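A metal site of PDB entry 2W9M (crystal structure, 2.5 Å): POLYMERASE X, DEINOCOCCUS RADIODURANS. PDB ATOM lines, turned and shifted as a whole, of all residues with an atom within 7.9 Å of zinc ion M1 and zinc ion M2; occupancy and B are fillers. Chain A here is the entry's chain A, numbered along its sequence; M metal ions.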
ATOM      1  N   GLY A  90      -6.350   1.215  23.064  1.00  0.00           N
ATOM      2  CA  GLY A  90      -7.041   2.022  24.042  1.00  0.00           C
ATOM      3  C   GLY A  90      -8.371   2.582  23.561  1.00  0.00           C
ATOM      4  O   GLY A  90      -9.192   3.034  24.369  1.00  0.00           O
ATOM      5  N   GLN A  91      -8.599   2.526  22.257  1.00  0.00           N
ATOM      6  CA  GLN A  91      -9.813   3.114  21.673  1.00  0.00           C
ATOM      7  C   GLN A  91     -10.861   2.076  21.306  1.00  0.00           C
ATOM      8  O   GLN A  91     -12.058   2.324  21.440  1.00  0.00           O
ATOM      9  CB  GLN A  91      -9.453   3.946  20.450  1.00  0.00           C
ATOM     10  CG  GLN A  91      -8.543   5.119  20.759  1.00  0.00           C
ATOM     11  CD  GLN A  91      -8.138   5.868  19.526  1.00  0.00           C
ATOM     12  OE1 GLN A  91      -8.821   5.806  18.501  1.00  0.00           O
ATOM     13  NE2 GLN A  91      -7.025   6.582  19.596  1.00  0.00           N
ATOM     14  N   LEU A  92     -10.396   0.918  20.839  1.00  0.00           N
ATOM     15  CA  LEU A  92     -11.298  -0.126  20.369  1.00  0.00           C
ATOM     16  C   LEU A  92     -12.055  -0.824  21.498  1.00  0.00           C
ATOM     17  O   LEU A  92     -11.557  -0.894  22.637  1.00  0.00           O
ATOM     18  CB  LEU A  92     -10.522  -1.150  19.533  1.00  0.00           C
ATOM     19  CG  LEU A  92     -10.006  -0.597  18.197  1.00  0.00           C
ATOM     20  CD1 LEU A  92      -9.149  -1.636  17.488  1.00  0.00           C
ATOM     21  CD2 LEU A  92     -11.153  -0.145  17.297  1.00  0.00           C
ATOM     22  N   PRO A  93     -13.255  -1.330  21.200  1.00  0.00           N
ATOM     23  CA  PRO A  93     -14.082  -2.048  22.174  1.00  0.00           C
ATOM     24  C   PRO A  93     -13.399  -3.344  22.587  1.00  0.00           C
ATOM     25  O   PRO A  93     -12.727  -3.963  21.771  1.00  0.00           O
ATOM     26  CB  PRO A  93     -15.354  -2.370  21.383  1.00  0.00           C
ATOM     27  CG  PRO A  93     -15.355  -1.424  20.228  1.00  0.00           C
ATOM     28  CD  PRO A  93     -13.918  -1.209  19.896  1.00  0.00           C
ATOM     29  N   PRO A  94     -13.595  -3.764  23.844  1.00  0.00           N
ATOM     30  CA  PRO A  94     -12.983  -4.984  24.397  1.00  0.00           C
ATOM     31  C   PRO A  94     -13.275  -6.217  23.556  1.00  0.00           C
ATOM     32  O   PRO A  94     -12.386  -7.024  23.318  1.00  0.00           O
ATOM     33  CB  PRO A  94     -13.667  -5.120  25.765  1.00  0.00           C
ATOM     34  CG  PRO A  94     -14.035  -3.731  26.132  1.00  0.00           C
ATOM     35  CD  PRO A  94     -14.414  -3.061  24.842  1.00  0.00           C
ATOM     36  N   HIS A 332     -25.267   6.028  26.794  1.00  0.00           N
ATOM     37  CA  HIS A 332     -23.923   5.636  26.413  1.00  0.00           C
ATOM     38  C   HIS A 332     -23.928   4.381  25.536  1.00  0.00           C
ATOM     39  O   HIS A 332     -23.471   3.319  25.928  1.00  0.00           O
ATOM     40  CB  HIS A 332     -23.040   5.451  27.646  1.00  0.00           C
ATOM     41  CG  HIS A 332     -21.591   5.241  27.321  1.00  0.00           C
ATOM     42  ND1 HIS A 332     -20.678   4.799  28.253  1.00  0.00           N
ATOM     43  CD2 HIS A 332     -20.905   5.393  26.168  1.00  0.00           C
ATOM     44  CE1 HIS A 332     -19.493   4.700  27.690  1.00  0.00           C
ATOM     45  NE2 HIS A 332     -19.603   5.057  26.420  1.00  0.00           N
ATOM     46  N   THR A 333     -24.474   4.527  24.332  1.00  0.00           N
ATOM     47  CA  THR A 333     -24.480   3.452  23.350  1.00  0.00           C
ATOM     48  C   THR A 333     -23.763   3.939  22.095  1.00  0.00           C
ATOM     49  O   THR A 333     -23.659   5.146  21.863  1.00  0.00           O
ATOM     50  CB  THR A 333     -25.914   3.050  22.980  1.00  0.00           C
ATOM     51  OG1 THR A 333     -26.577   4.177  22.396  1.00  0.00           O
ATOM     52  CG2 THR A 333     -26.682   2.598  24.208  1.00  0.00           C
ATOM     53  N   HIS A 334     -23.269   3.017  21.275  1.00  0.00           N
ATOM     54  CA  HIS A 334     -22.548   3.387  20.056  1.00  0.00           C
ATOM     55  C   HIS A 334     -23.271   2.917  18.795  1.00  0.00           C
ATOM     56  O   HIS A 334     -23.967   1.903  18.812  1.00  0.00           O
ATOM     57  CB  HIS A 334     -21.115   2.872  20.081  1.00  0.00           C
ATOM     58  CG  HIS A 334     -20.274   3.506  21.142  1.00  0.00           C
ATOM     59  ND1 HIS A 334     -19.372   4.519  20.881  1.00  0.00           N
ATOM     60  CD2 HIS A 334     -20.208   3.287  22.480  1.00  0.00           C
ATOM     61  CE1 HIS A 334     -18.783   4.894  21.999  1.00  0.00           C
ATOM     62  NE2 HIS A 334     -19.282   4.155  22.993  1.00  0.00           N
ATOM     63  N   SER A 338     -19.897   5.796  14.692  1.00  0.00           N
ATOM     64  CA  SER A 338     -18.625   5.663  15.375  1.00  0.00           C
ATOM     65  C   SER A 338     -18.026   4.280  15.079  1.00  0.00           C
ATOM     66  O   SER A 338     -17.720   3.954  13.926  1.00  0.00           O
ATOM     67  CB  SER A 338     -18.822   5.833  16.875  1.00  0.00           C
ATOM     68  OG  SER A 338     -17.635   6.244  17.519  1.00  0.00           O
ATOM     69  N   ASP A 339     -17.860   3.480  16.120  1.00  0.00           N
ATOM     70  CA  ASP A 339     -17.370   2.117  15.964  1.00  0.00           C
ATOM     71  C   ASP A 339     -18.411   1.072  16.367  1.00  0.00           C
ATOM     72  O   ASP A 339     -18.069  -0.031  16.766  1.00  0.00           O
ATOM     73  CB  ASP A 339     -16.065   1.914  16.740  1.00  0.00           C
ATOM     74  CG  ASP A 339     -16.242   2.068  18.240  1.00  0.00           C
ATOM     75  OD1 ASP A 339     -17.307   2.569  18.674  1.00  0.00           O
ATOM     76  OD2 ASP A 339     -15.318   1.687  18.996  1.00  0.00           O
ATOM     77  N   ALA A 362     -24.201   8.165  22.121  1.00  0.00           N
ATOM     78  CA  ALA A 362     -22.901   8.543  22.686  1.00  0.00           C
ATOM     79  C   ALA A 362     -21.700   7.970  21.918  1.00  0.00           C
ATOM     80  O   ALA A 362     -20.942   7.178  22.460  1.00  0.00           O
ATOM     81  CB  ALA A 362     -22.818   8.152  24.152  1.00  0.00           C
ATOM     82  N   ASP A 363     -21.547   8.386  20.672  1.00  0.00           N
ATOM     83  CA  ASP A 363     -20.427   7.928  19.847  1.00  0.00           C
ATOM     84  C   ASP A 363     -19.154   8.696  20.193  1.00  0.00           C
ATOM     85  O   ASP A 363     -19.210   9.755  20.810  1.00  0.00           O
ATOM     86  CB  ASP A 363     -20.782   8.066  18.353  1.00  0.00           C
ATOM     87  CG  ASP A 363     -21.742   6.981  17.884  1.00  0.00           C
ATOM     88  OD1 ASP A 363     -21.370   5.793  17.936  1.00  0.00           O
ATOM     89  OD2 ASP A 363     -22.877   7.318  17.477  1.00  0.00           O
ATOM     90  N   HIS A 364     -18.002   8.155  19.809  1.00  0.00           N
ATOM     91  CA  HIS A 364     -16.722   8.785  20.147  1.00  0.00           C
ATOM     92  C   HIS A 364     -16.531  10.075  19.383  1.00  0.00           C
ATOM     93  O   HIS A 364     -17.274  10.390  18.447  1.00  0.00           O
ATOM     94  CB  HIS A 364     -15.547   7.854  19.825  1.00  0.00           C
ATOM     95  CG  HIS A 364     -15.667   6.493  20.413  1.00  0.00           C
ATOM     96  ND1 HIS A 364     -15.218   6.181  21.680  1.00  0.00           N
ATOM     97  CD2 HIS A 364     -16.199   5.354  19.903  1.00  0.00           C
ATOM     98  CE1 HIS A 364     -15.467   4.905  21.922  1.00  0.00           C
ATOM     99  NE2 HIS A 364     -16.063   4.387  20.870  1.00  0.00           N
ATOM    100  N   GLU A 401     -19.504  10.635  23.565  1.00  0.00           N
ATOM    101  CA  GLU A 401     -18.453  10.232  24.486  1.00  0.00           C
ATOM    102  C   GLU A 401     -17.203  11.027  24.161  1.00  0.00           C
ATOM    103  O   GLU A 401     -16.399  10.632  23.314  1.00  0.00           O
ATOM    104  CB  GLU A 401     -18.170   8.735  24.416  1.00  0.00           C
ATOM    105  CG  GLU A 401     -17.224   8.277  25.519  1.00  0.00           C
ATOM    106  CD  GLU A 401     -16.901   6.812  25.470  1.00  0.00           C
ATOM    107  OE1 GLU A 401     -17.447   6.120  24.578  1.00  0.00           O
ATOM    108  OE2 GLU A 401     -16.102   6.356  26.322  1.00  0.00           O
ATOM    109  N   VAL A 424     -20.820  12.506  28.002  1.00  0.00           N
ATOM    110  CA  VAL A 424     -20.009  11.531  28.731  1.00  0.00           C
ATOM    111  C   VAL A 424     -18.542  11.852  28.477  1.00  0.00           C
ATOM    112  O   VAL A 424     -18.162  12.149  27.350  1.00  0.00           O
ATOM    113  CB  VAL A 424     -20.294  10.077  28.258  1.00  0.00           C
ATOM    114  CG1 VAL A 424     -19.389   9.077  28.990  1.00  0.00           C
ATOM    115  CG2 VAL A 424     -21.755   9.710  28.445  1.00  0.00           C
ATOM    116  N   VAL A 425     -17.720  11.821  29.520  1.00  0.00           N
ATOM    117  CA  VAL A 425     -16.279  11.989  29.353  1.00  0.00           C
ATOM    118  C   VAL A 425     -15.536  10.716  29.706  1.00  0.00           C
ATOM    119  O   VAL A 425     -15.931   9.983  30.614  1.00  0.00           O
ATOM    120  CB  VAL A 425     -15.718  13.168  30.188  1.00  0.00           C
ATOM    121  CG1 VAL A 425     -16.420  14.453  29.796  1.00  0.00           C
ATOM    122  CG2 VAL A 425     -15.876  12.886  31.667  1.00  0.00           C
ATOM    123  N   SER A 426     -14.453  10.444  28.985  1.00  0.00           N
ATOM    124  CA  SER A 426     -13.738   9.180  29.127  1.00  0.00           C
ATOM    125  C   SER A 426     -12.292   9.285  28.675  1.00  0.00           C
ATOM    126  O   SER A 426     -11.961  10.109  27.836  1.00  0.00           O
ATOM    127  CB  SER A 426     -14.437   8.089  28.309  1.00  0.00           C
ATOM    128  OG  SER A 426     -15.759   7.858  28.778  1.00  0.00           O
ATOM    129  N   VAL A 427     -11.445   8.429  29.245  1.00  0.00           N
ATOM    130  CA  VAL A 427     -10.065   8.296  28.804  1.00  0.00           C
ATOM    131  C   VAL A 427      -9.957   7.160  27.788  1.00  0.00           C
ATOM    132  O   VAL A 427     -10.445   6.056  28.020  1.00  0.00           O
ATOM    133  CB  VAL A 427      -9.126   7.990  29.989  1.00  0.00           C
ATOM    134  CG1 VAL A 427      -7.683   7.932  29.513  1.00  0.00           C
ATOM    135  CG2 VAL A 427      -9.282   9.038  31.072  1.00  0.00           C
ATOM    136  N   HIS A 428      -9.315   7.436  26.652  1.00  0.00           N
ATOM    137  CA  HIS A 428      -9.088   6.441  25.623  1.00  0.00           C
ATOM    138  C   HIS A 428      -7.667   6.561  25.059  1.00  0.00           C
ATOM    139  O   HIS A 428      -7.334   5.983  24.014  1.00  0.00           O
ATOM    140  CB  HIS A 428     -10.104   6.588  24.492  1.00  0.00           C
ATOM    141  CG  HIS A 428     -11.455   6.023  24.809  1.00  0.00           C
ATOM    142  ND1 HIS A 428     -11.671   4.670  24.991  1.00  0.00           N
ATOM    143  CD2 HIS A 428     -12.657   6.619  24.947  1.00  0.00           C
ATOM    144  CE1 HIS A 428     -12.952   4.469  25.248  1.00  0.00           C
ATOM    145  NE2 HIS A 428     -13.568   5.641  25.236  1.00  0.00           N
ATOM    146  N   GLY A 455     -17.308   8.258  32.175  1.00  0.00           N
ATOM    147  CA  GLY A 455     -17.292   6.907  31.631  1.00  0.00           C
ATOM    148  C   GLY A 455     -16.215   6.021  32.252  1.00  0.00           C
ATOM    149  O   GLY A 455     -15.165   6.521  32.657  1.00  0.00           O
ATOM    150  N   HIS A 456     -16.474   4.718  32.314  1.00  0.00           N
ATOM    151  CA  HIS A 456     -15.560   3.715  32.894  1.00  0.00           C
ATOM    152  C   HIS A 456     -14.321   4.301  33.582  1.00  0.00           C
ATOM    153  O   HIS A 456     -13.220   4.274  33.023  1.00  0.00           O
ATOM    154  CB  HIS A 456     -15.145   2.689  31.839  1.00  0.00           C
ATOM    155  CG  HIS A 456     -14.811   3.306  30.517  1.00  0.00           C
ATOM    156  ND1 HIS A 456     -13.621   3.970  30.284  1.00  0.00           N
ATOM    157  CD2 HIS A 456     -15.507   3.366  29.363  1.00  0.00           C
ATOM    158  CE1 HIS A 456     -13.604   4.405  29.038  1.00  0.00           C
ATOM    159  NE2 HIS A 456     -14.735   4.053  28.453  1.00  0.00           N
ATOM    160  N   GLU A 487     -20.110   6.426  36.114  1.00  0.00           N
ATOM    161  CA  GLU A 487     -20.671   5.302  35.379  1.00  0.00           C
ATOM    162  C   GLU A 487     -20.232   3.957  35.957  1.00  0.00           C
ATOM    163  O   GLU A 487     -19.080   3.781  36.348  1.00  0.00           O
ATOM    164  CB  GLU A 487     -20.270   5.384  33.901  1.00  0.00           C
ATOM    165  CG  GLU A 487     -20.496   4.111  33.083  1.00  0.00           C
ATOM    166  CD  GLU A 487     -20.222   4.323  31.596  1.00  0.00           C
ATOM    167  OE1 GLU A 487     -21.088   4.927  30.922  1.00  0.00           O
ATOM    168  OE2 GLU A 487     -19.160   3.877  31.105  1.00  0.00           O
ATOM    169  N   ASN A 489     -19.958   0.768  34.196  1.00  0.00           N
ATOM    170  CA  ASN A 489     -20.025   0.246  32.844  1.00  0.00           C
ATOM    171  C   ASN A 489     -20.401  -1.216  32.860  1.00  0.00           C
ATOM    172  O   ASN A 489     -19.671  -2.058  33.381  1.00  0.00           O
ATOM    173  CB  ASN A 489     -18.690   0.479  32.133  1.00  0.00           C
ATOM    174  CG  ASN A 489     -18.799   0.349  30.624  1.00  0.00           C
ATOM    175  OD1 ASN A 489     -19.065  -0.733  30.108  1.00  0.00           O
ATOM    176  ND2 ASN A 489     -18.578   1.451  29.922  1.00  0.00           N
ATOM    177  N   ARG A 494     -15.536  -4.731  31.344  1.00  0.00           N
ATOM    178  CA  ARG A 494     -15.204  -3.542  32.113  1.00  0.00           C
ATOM    179  C   ARG A 494     -15.668  -3.632  33.567  1.00  0.00           C
ATOM    180  O   ARG A 494     -14.847  -3.646  34.481  1.00  0.00           O
ATOM    181  CB  ARG A 494     -15.753  -2.280  31.439  1.00  0.00           C
ATOM    182  CG  ARG A 494     -15.074  -1.971  30.122  1.00  0.00           C
ATOM    183  CD  ARG A 494     -15.633  -0.695  29.507  1.00  0.00           C
ATOM    184  NE  ARG A 494     -15.085  -0.436  28.175  1.00  0.00           N
ATOM    185  CZ  ARG A 494     -13.889   0.090  27.954  1.00  0.00           C
ATOM    186  NH1 ARG A 494     -13.090   0.402  28.965  1.00  0.00           N
ATOM    187  NH2 ARG A 494     -13.487   0.295  26.704  1.00  0.00           N
ATOM    188  N   THR A 515     -24.512   0.305  29.404  1.00  0.00           N
ATOM    189  CA  THR A 515     -24.065  -0.904  28.719  1.00  0.00           C
ATOM    190  C   THR A 515     -22.853  -0.656  27.803  1.00  0.00           C
ATOM    191  O   THR A 515     -22.072  -1.577  27.549  1.00  0.00           O
ATOM    192  CB  THR A 515     -25.204  -1.489  27.869  1.00  0.00           C
ATOM    193  OG1 THR A 515     -25.631  -0.511  26.920  1.00  0.00           O
ATOM    194  CG2 THR A 515     -26.370  -1.884  28.745  1.00  0.00           C
ATOM    195  N   ASP A 516     -22.712   0.572  27.318  1.00  0.00           N
ATOM    196  CA  ASP A 516     -21.668   0.888  26.340  1.00  0.00           C
ATOM    197  C   ASP A 516     -21.811  -0.013  25.119  1.00  0.00           C
ATOM    198  O   ASP A 516     -20.822  -0.419  24.515  1.00  0.00           O
ATOM    199  CB  ASP A 516     -20.284   0.720  26.969  1.00  0.00           C
ATOM    200  CG  ASP A 516     -19.210   1.504  26.234  1.00  0.00           C
ATOM    201  OD1 ASP A 516     -19.522   2.069  25.170  1.00  0.00           O
ATOM    202  OD2 ASP A 516     -18.060   1.554  26.724  1.00  0.00           O
ATOM    203  N   ALA A 517     -23.053  -0.307  24.747  1.00  0.00           N
ATOM    204  CA  ALA A 517     -23.346  -1.214  23.631  1.00  0.00           C
ATOM    205  C   ALA A 517     -22.791  -0.733  22.290  1.00  0.00           C
ATOM    206  O   ALA A 517     -23.045   0.399  21.859  1.00  0.00           O
ATOM    207  CB  ALA A 517     -24.848  -1.451  23.521  1.00  0.00           C
ATOM    208  N   HIS A 518     -22.033  -1.591  21.616  1.00  0.00           N
ATOM    209  CA  HIS A 518     -21.554  -1.308  20.278  1.00  0.00           C
ATOM    210  C   HIS A 518     -22.367  -2.079  19.235  1.00  0.00           C
ATOM    211  O   HIS A 518     -22.094  -2.021  18.042  1.00  0.00           O
ATOM    212  CB  HIS A 518     -20.069  -1.650  20.159  1.00  0.00           C
ATOM    213  CG  HIS A 518     -19.176  -0.650  20.811  1.00  0.00           C
ATOM    214  ND1 HIS A 518     -19.050  -0.538  22.176  1.00  0.00           N
ATOM    215  CD2 HIS A 518     -18.377   0.308  20.288  1.00  0.00           C
ATOM    216  CE1 HIS A 518     -18.210   0.430  22.471  1.00  0.00           C
ATOM    217  NE2 HIS A 518     -17.780   0.973  21.338  1.00  0.00           N
HETATM  218 ZN    ZN M   1     -18.162   4.042  24.993  1.00  0.00          ZN
HETATM  219 ZN    ZN M   2     -15.428   4.355  26.148  1.00  0.00          ZN
HETATM  220 ZN    ZN M   3     -16.228   2.331  20.991  1.00  0.00          ZN
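The side-chain carboxylate of Glu 401 lies close to the side-chain hydroxyl of Ser 426 (2.9 Å).
N of Glu 401 is in hydrogen-bond range of O of Asp 363, at 2.9 Å.
ND1 of His 334 sits close to NE2 of His 364 (3.3 Å).
The backbone carbonyl oxygen (O) of Ala 362 sits close to a ring nitrogen (ND1) of His 334, 3.5 Å away.
The backbone NH (N) of His 334 is in hydrogen-bond range of the backbone carbonyl oxygen (O) of Ala 517 (2.7 Å).
A ring nitrogen (ND1) of His 518 sits at hydrogen-bond distance from the backbone carbonyl oxygen (O) of Asp 516 (2.9 Å).
The backbone NH (N) of His 456 is in hydrogen-bond range of the side-chain carboxylate (OE2) of Glu 487, 3.1 Å away.
A ring nitrogen (ND1) of His 428 is in hydrogen-bond range of the backbone carbonyl oxygen of Gly 90 (3.0 Å).
Within 4 Å of zinc ion M2: Glu 401, His 428, His 456 and Asp 516.
The nearest printed residue that does not touch zinc ion M2 is His 332 (4.2 Å).
Zinc ion M1 is bound by the side-chain carboxylate of Glu 401 (2.2 Å), a ring nitrogen (NE2) of His 332 (2.3 Å), a ring nitrogen (NE2) of His 334 (2.3 Å) and the side-chain carboxylate of Asp 516 (2.4 Å).
The side-chain carboxylate (OE2) of Glu 401 is bound to zinc ion M2, at 2.1 Å.
Zinc ion M2 is bound by NE2 of His 456, at 2.4 Å.
Zinc ion M2 is bound by NE2 of His 428.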
